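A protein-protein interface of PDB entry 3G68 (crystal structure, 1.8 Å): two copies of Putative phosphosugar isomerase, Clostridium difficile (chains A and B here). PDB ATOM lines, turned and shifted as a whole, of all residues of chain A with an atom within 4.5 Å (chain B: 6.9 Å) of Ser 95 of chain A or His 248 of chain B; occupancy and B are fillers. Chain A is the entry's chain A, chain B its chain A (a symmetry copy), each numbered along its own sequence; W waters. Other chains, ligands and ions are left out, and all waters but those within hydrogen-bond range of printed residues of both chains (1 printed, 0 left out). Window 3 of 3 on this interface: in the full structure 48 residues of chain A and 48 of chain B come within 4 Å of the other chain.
OG of Ser 42 of chain A sits at hydrogen-bond distance from OG of Ser 97 of chain A, 2.6 Å away. OE2 of Glu 244 of chain B is in hydrogen-bond range of NE2 of His 248 of chain B (3.3 Å). The backbone carbonyl oxygen (O) of Gly 249 of chain B lies close to the side-chain amide oxygen (OD1) of Asn 252 of chain B, at 3.0 Å.
CB of Ser 42 of chain A touches CE1 of His 248 of chain B (3.6 Å). CE1 of His 248 of chain B touches OG of Ser 95 of chain A, at 3.5 Å. Ser 97 of chain A touches Glu 244 of chain B (CB to CG, 3.6 Å). His 248 of chain B touches Ser 97 of chain A. Leu 228 of chain A touches Ile 250 of chain B. O of His 248 of chain B touches OE2 of Glu 232 of chain A (3.8 Å). Gly 249 of chain B touches Glu 232 of chain A (CA to OE2, 3.5 Å). Glu 232 of chain A touches Asn 252 of chain B.
Water W1 lies within hydrogen-bond range of OE2 of Glu 244 of chain B (2.5 Å), NE2 of His 248 of chain B (2.9 Å), OG of Ser 97 of chain A (3.1 Å) and N of Tyr 96 of chain A (3.5 Å).
Hydrophobic or aromatic side chains of chain B within 4 Å of the printed part of chain A: His 248 and Ile 250. Of the 11 printed residues of chain A, 5 touch a printed residue of chain B. Among the printed residues, 9 pairs touch across the chains. Among the printed residues, no Asp or Glu carboxylate lies within 4 Å of a Lys or Arg side-chain nitrogen of the other chain.
Of chain B, only His 248 (3.5 Å) comes within 4 Å of Ser 95 of chain A. His 248 of chain B touches four residues of chain A. Printed residues of chain A within 4 Å of Glu 244 of chain B: Ser 97. Printed residues of chain B within 4 Å of Leu 228 of chain A: Ile 250. Of the printed residues of chain A, Asn 252 of chain B touches Glu 232 (3.8 Å). Of the printed residues of chain A, Ile 250 of chain B touches Leu 228 (3.5 Å). Gly 93 of chain A touches none of the printed residues of chain B. Tyr 96 of chain A touches none of the printed residues of chain B. The nearest residue of chain A that does not touch His 248 of chain B is Leu 228 of chain A (4.2 Å).
The side-chain hydroxyl (OG) of Ser 42 of chain A lies within hydrogen-bond range of the side-chain carboxylate (OE2) of Glu 245 of chain B (2.7 Å).
No position is printed for both chains. Of the 9 pairs that touch across the chains among the printed residues, none has its exchanged pair printed and touching as well.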
ATOM      1  N   SER A  42     -16.755  27.049  17.514  1.00  0.00           N
ATOM      2  CA  SER A  42     -17.511  26.482  18.623  1.00  0.00           C
ATOM      3  C   SER A  42     -18.998  26.635  18.385  1.00  0.00           C
ATOM      4  O   SER A  42     -19.432  27.518  17.635  1.00  0.00           O
ATOM      5  CB  SER A  42     -17.130  27.141  19.952  1.00  0.00           C
ATOM      6  OG  SER A  42     -15.823  26.753  20.338  1.00  0.00           O
ATOM      7  N   SER A  90     -16.446  32.422  13.862  1.00  0.00           N
ATOM      8  CA  SER A  90     -16.971  32.931  15.115  1.00  0.00           C
ATOM      9  C   SER A  90     -17.814  34.143  14.824  1.00  0.00           C
ATOM     10  O   SER A  90     -17.275  35.162  14.428  1.00  0.00           O
ATOM     11  CB  SER A  90     -15.845  33.339  16.044  1.00  0.00           C
ATOM     12  OG  SER A  90     -16.405  33.938  17.200  1.00  0.00           O
ATOM     13  N   GLY A  93     -16.903  36.931  16.854  1.00  0.00           N
ATOM     14  CA  GLY A  93     -15.538  37.182  16.463  1.00  0.00           C
ATOM     15  C   GLY A  93     -14.515  37.109  17.567  1.00  0.00           C
ATOM     16  O   GLY A  93     -13.351  37.263  17.275  1.00  0.00           O
ATOM     17  N   SER A  94     -14.945  36.843  18.804  1.00  0.00           N
ATOM     18  CA  SER A  94     -14.055  36.834  19.961  1.00  0.00           C
ATOM     19  C   SER A  94     -14.035  35.568  20.824  1.00  0.00           C
ATOM     20  O   SER A  94     -13.569  35.623  21.973  1.00  0.00           O
ATOM     21  CB  SER A  94     -14.435  38.036  20.831  1.00  0.00           C
ATOM     22  OG  SER A  94     -15.796  37.938  21.210  1.00  0.00           O
ATOM     23  N   SER A  95     -14.509  34.434  20.303  1.00  0.00           N
ATOM     24  CA  SER A  95     -14.492  33.184  21.074  1.00  0.00           C
ATOM     25  C   SER A  95     -13.033  32.768  21.269  1.00  0.00           C
ATOM     26  O   SER A  95     -12.313  32.608  20.294  1.00  0.00           O
ATOM     27  CB  SER A  95     -15.305  32.077  20.377  1.00  0.00           C
ATOM     28  OG  SER A  95     -16.693  32.365  20.401  1.00  0.00           O
ATOM     29  N   TYR A  96     -12.590  32.634  22.521  1.00  0.00           N
ATOM     30  CA  TYR A  96     -11.192  32.250  22.775  1.00  0.00           C
ATOM     31  C   TYR A  96     -10.861  30.833  22.331  1.00  0.00           C
ATOM     32  O   TYR A  96      -9.728  30.573  21.990  1.00  0.00           O
ATOM     33  CB  TYR A  96     -10.790  32.429  24.247  1.00  0.00           C
ATOM     34  CG  TYR A  96     -10.822  33.863  24.753  1.00  0.00           C
ATOM     35  CD1 TYR A  96     -10.181  34.903  24.049  1.00  0.00           C
ATOM     36  CD2 TYR A  96     -11.433  34.173  25.982  1.00  0.00           C
ATOM     37  CE1 TYR A  96     -10.193  36.217  24.530  1.00  0.00           C
ATOM     38  CE2 TYR A  96     -11.450  35.477  26.477  1.00  0.00           C
ATOM     39  CZ  TYR A  96     -10.826  36.493  25.755  1.00  0.00           C
ATOM     40  OH  TYR A  96     -10.858  37.780  26.258  1.00  0.00           O
ATOM     41  N   SER A  97     -11.838  29.923  22.367  1.00  0.00           N
ATOM     42  CA  SER A  97     -11.643  28.548  21.893  1.00  0.00           C
ATOM     43  C   SER A  97     -11.111  28.609  20.455  1.00  0.00           C
ATOM     44  O   SER A  97     -10.043  28.067  20.151  1.00  0.00           O
ATOM     45  CB  SER A  97     -12.971  27.733  21.945  1.00  0.00           C
ATOM     46  OG  SER A  97     -14.097  28.439  21.360  1.00  0.00           O
ATOM     47  N   THR A  98     -11.850  29.323  19.600  1.00  0.00           N
ATOM     48  CA  THR A  98     -11.531  29.466  18.151  1.00  0.00           C
ATOM     49  C   THR A  98     -10.263  30.290  17.917  1.00  0.00           C
ATOM     50  O   THR A  98      -9.404  29.913  17.123  1.00  0.00           O
ATOM     51  CB  THR A  98     -12.747  30.041  17.426  1.00  0.00           C
ATOM     52  OG1 THR A  98     -13.886  29.213  17.746  1.00  0.00           O
ATOM     53  CG2 THR A  98     -12.566  30.139  15.869  1.00  0.00           C
ATOM     54  N   TYR A  99     -10.129  31.387  18.661  1.00  0.00           N
ATOM     55  CA  TYR A  99      -8.938  32.210  18.580  1.00  0.00           C
ATOM     56  C   TYR A  99      -7.697  31.341  18.892  1.00  0.00           C
ATOM     57  O   TYR A  99      -6.718  31.380  18.137  1.00  0.00           O
ATOM     58  CB  TYR A  99      -9.054  33.364  19.583  1.00  0.00           C
ATOM     59  CG  TYR A  99      -7.910  34.355  19.530  1.00  0.00           C
ATOM     60  CD1 TYR A  99      -6.682  34.082  20.143  1.00  0.00           C
ATOM     61  CD2 TYR A  99      -8.058  35.570  18.873  1.00  0.00           C
ATOM     62  CE1 TYR A  99      -5.623  35.008  20.087  1.00  0.00           C
ATOM     63  CE2 TYR A  99      -7.005  36.502  18.822  1.00  0.00           C
ATOM     64  CZ  TYR A  99      -5.796  36.217  19.420  1.00  0.00           C
ATOM     65  OH  TYR A  99      -4.759  37.155  19.357  1.00  0.00           O
ATOM     66  N   LEU A 228     -29.352  22.568  19.344  1.00  0.00           N
ATOM     67  CA  LEU A 228     -28.724  23.551  20.221  1.00  0.00           C
ATOM     68  C   LEU A 228     -29.608  24.785  20.432  1.00  0.00           C
ATOM     69  O   LEU A 228     -29.730  25.276  21.566  1.00  0.00           O
ATOM     70  CB  LEU A 228     -27.343  23.991  19.723  1.00  0.00           C
ATOM     71  CG  LEU A 228     -26.644  25.064  20.551  1.00  0.00           C
ATOM     72  CD1 LEU A 228     -26.394  24.597  22.040  1.00  0.00           C
ATOM     73  CD2 LEU A 228     -25.343  25.494  19.879  1.00  0.00           C
ATOM     74  N   GLU A 232     -31.180  26.143  24.026  1.00  0.00           N
ATOM     75  CA  GLU A 232     -30.896  27.463  24.546  1.00  0.00           C
ATOM     76  C   GLU A 232     -32.141  28.287  24.827  1.00  0.00           C
ATOM     77  O   GLU A 232     -32.149  29.099  25.764  1.00  0.00           O
ATOM     78  CB  GLU A 232     -29.979  28.249  23.576  1.00  0.00           C
ATOM     79  CG  GLU A 232     -28.566  27.724  23.475  1.00  0.00           C
ATOM     80  CD  GLU A 232     -27.727  28.397  22.400  1.00  0.00           C
ATOM     81  OE1 GLU A 232     -28.268  29.158  21.580  1.00  0.00           O
ATOM     82  OE2 GLU A 232     -26.500  28.143  22.368  1.00  0.00           O
ATOM     83  N   PHE B 243     -15.888  20.370  27.938  1.00  0.00           N
ATOM     84  CA  PHE B 243     -16.009  21.504  28.864  1.00  0.00           C
ATOM     85  C   PHE B 243     -16.199  22.869  28.195  1.00  0.00           C
ATOM     86  O   PHE B 243     -17.112  23.622  28.527  1.00  0.00           O
ATOM     87  CB  PHE B 243     -14.752  21.522  29.774  1.00  0.00           C
ATOM     88  CG  PHE B 243     -14.840  22.468  30.917  1.00  0.00           C
ATOM     89  CD1 PHE B 243     -14.501  23.802  30.754  1.00  0.00           C
ATOM     90  CD2 PHE B 243     -15.211  22.012  32.185  1.00  0.00           C
ATOM     91  CE1 PHE B 243     -14.557  24.669  31.805  1.00  0.00           C
ATOM     92  CE2 PHE B 243     -15.275  22.895  33.266  1.00  0.00           C
ATOM     93  CZ  PHE B 243     -14.948  24.222  33.076  1.00  0.00           C
ATOM     94  N   GLU B 244     -15.297  23.211  27.287  1.00  0.00           N
ATOM     95  CA  GLU B 244     -15.404  24.485  26.563  1.00  0.00           C
ATOM     96  C   GLU B 244     -16.683  24.577  25.751  1.00  0.00           C
ATOM     97  O   GLU B 244     -17.297  25.626  25.727  1.00  0.00           O
ATOM     98  CB  GLU B 244     -14.147  24.742  25.701  1.00  0.00           C
ATOM     99  CG  GLU B 244     -14.124  26.080  24.986  1.00  0.00           C
ATOM    100  CD  GLU B 244     -14.207  27.279  25.907  1.00  0.00           C
ATOM    101  OE1 GLU B 244     -13.578  27.253  26.974  1.00  0.00           O
ATOM    102  OE2 GLU B 244     -14.902  28.256  25.555  1.00  0.00           O
ATOM    103  N   GLU B 245     -17.125  23.496  25.116  1.00  0.00           N
ATOM    104  CA  GLU B 245     -18.361  23.529  24.340  1.00  0.00           C
ATOM    105  C   GLU B 245     -19.601  23.679  25.230  1.00  0.00           C
ATOM    106  O   GLU B 245     -20.544  24.393  24.866  1.00  0.00           O
ATOM    107  CB  GLU B 245     -18.447  22.343  23.370  1.00  0.00           C
ATOM    108  CG  GLU B 245     -17.328  22.359  22.281  1.00  0.00           C
ATOM    109  CD  GLU B 245     -17.314  23.623  21.434  1.00  0.00           C
ATOM    110  OE1 GLU B 245     -18.378  23.889  20.819  1.00  0.00           O
ATOM    111  OE2 GLU B 245     -16.242  24.334  21.382  1.00  0.00           O
ATOM    112  N   PHE B 246     -19.557  23.117  26.439  1.00  0.00           N
ATOM    113  CA  PHE B 246     -20.633  23.315  27.383  1.00  0.00           C
ATOM    114  C   PHE B 246     -20.825  24.788  27.694  1.00  0.00           C
ATOM    115  O   PHE B 246     -21.946  25.249  27.868  1.00  0.00           O
ATOM    116  CB  PHE B 246     -20.372  22.556  28.685  1.00  0.00           C
ATOM    117  CG  PHE B 246     -21.522  22.608  29.669  1.00  0.00           C
ATOM    118  CD1 PHE B 246     -21.615  23.632  30.609  1.00  0.00           C
ATOM    119  CD2 PHE B 246     -22.506  21.611  29.687  1.00  0.00           C
ATOM    120  CE1 PHE B 246     -22.664  23.690  31.526  1.00  0.00           C
ATOM    121  CE2 PHE B 246     -23.571  21.671  30.593  1.00  0.00           C
ATOM    122  CZ  PHE B 246     -23.624  22.703  31.546  1.00  0.00           C
ATOM    123  N   ILE B 247     -19.714  25.529  27.762  1.00  0.00           N
ATOM    124  CA  ILE B 247     -19.768  26.959  28.042  1.00  0.00           C
ATOM    125  C   ILE B 247     -20.509  27.741  26.956  1.00  0.00           C
ATOM    126  O   ILE B 247     -21.152  28.757  27.249  1.00  0.00           O
ATOM    127  CB  ILE B 247     -18.329  27.522  28.297  1.00  0.00           C
ATOM    128  CG1 ILE B 247     -17.763  26.876  29.567  1.00  0.00           C
ATOM    129  CG2 ILE B 247     -18.345  29.084  28.345  1.00  0.00           C
ATOM    130  CD1 ILE B 247     -16.263  27.133  29.785  1.00  0.00           C
ATOM    131  N   HIS B 248     -20.486  27.218  25.729  1.00  0.00           N
ATOM    132  CA  HIS B 248     -21.194  27.794  24.570  1.00  0.00           C
ATOM    133  C   HIS B 248     -22.686  27.447  24.483  1.00  0.00           C
ATOM    134  O   HIS B 248     -23.121  26.755  23.564  1.00  0.00           O
ATOM    135  CB  HIS B 248     -20.468  27.432  23.250  1.00  0.00           C
ATOM    136  CG  HIS B 248     -19.175  28.155  23.072  1.00  0.00           C
ATOM    137  ND1 HIS B 248     -19.075  29.324  22.349  1.00  0.00           N
ATOM    138  CD2 HIS B 248     -17.945  27.918  23.587  1.00  0.00           C
ATOM    139  CE1 HIS B 248     -17.823  29.750  22.386  1.00  0.00           C
ATOM    140  NE2 HIS B 248     -17.121  28.928  23.153  1.00  0.00           N
ATOM    141  N   GLY B 249     -23.430  27.902  25.487  1.00  0.00           N
ATOM    142  CA  GLY B 249     -24.881  27.820  25.509  1.00  0.00           C
ATOM    143  C   GLY B 249     -25.580  26.736  26.292  1.00  0.00           C
ATOM    144  O   GLY B 249     -26.757  26.869  26.588  1.00  0.00           O
ATOM    145  N   ILE B 250     -24.879  25.669  26.653  1.00  0.00           N
ATOM    146  CA  ILE B 250     -25.560  24.549  27.313  1.00  0.00           C
ATOM    147  C   ILE B 250     -26.070  24.893  28.707  1.00  0.00           C
ATOM    148  O   ILE B 250     -27.127  24.383  29.102  1.00  0.00           O
ATOM    149  CB  ILE B 250     -24.699  23.238  27.308  1.00  0.00           C
ATOM    150  CG1 ILE B 250     -24.152  22.945  25.899  1.00  0.00           C
ATOM    151  CG2 ILE B 250     -25.506  22.008  27.882  1.00  0.00           C
ATOM    152  CD1 ILE B 250     -25.175  22.847  24.772  1.00  0.00           C
ATOM    153  N   TYR B 251     -25.361  25.779  29.424  1.00  0.00           N
ATOM    154  CA  TYR B 251     -25.748  26.225  30.783  1.00  0.00           C
ATOM    155  C   TYR B 251     -27.180  26.774  30.835  1.00  0.00           C
ATOM    156  O   TYR B 251     -27.820  26.711  31.869  1.00  0.00           O
ATOM    157  CB  TYR B 251     -24.771  27.285  31.318  1.00  0.00           C
ATOM    158  CG  TYR B 251     -24.788  28.557  30.518  1.00  0.00           C
ATOM    159  CD1 TYR B 251     -23.966  28.710  29.401  1.00  0.00           C
ATOM    160  CD2 TYR B 251     -25.614  29.614  30.876  1.00  0.00           C
ATOM    161  CE1 TYR B 251     -23.987  29.880  28.659  1.00  0.00           C
ATOM    162  CE2 TYR B 251     -25.650  30.772  30.128  1.00  0.00           C
ATOM    163  CZ  TYR B 251     -24.839  30.912  29.034  1.00  0.00           C
ATOM    164  OH  TYR B 251     -24.855  32.091  28.299  1.00  0.00           O
ATOM    165  N   ASN B 252     -27.673  27.306  29.708  1.00  0.00           N
ATOM    166  CA  ASN B 252     -29.026  27.844  29.620  1.00  0.00           C
ATOM    167  C   ASN B 252     -30.111  26.860  30.024  1.00  0.00           C
ATOM    168  O   ASN B 252     -31.154  27.285  30.491  1.00  0.00           O
ATOM    169  CB  ASN B 252     -29.338  28.269  28.164  1.00  0.00           C
ATOM    170  CG  ASN B 252     -28.683  29.552  27.775  1.00  0.00           C
ATOM    171  OD1 ASN B 252     -27.883  29.613  26.827  1.00  0.00           O
ATOM    172  ND2 ASN B 252     -28.980  30.600  28.524  1.00  0.00           N
HETATM  173  O   HOH W   1     -14.583  30.104  23.885  1.00  0.00           O
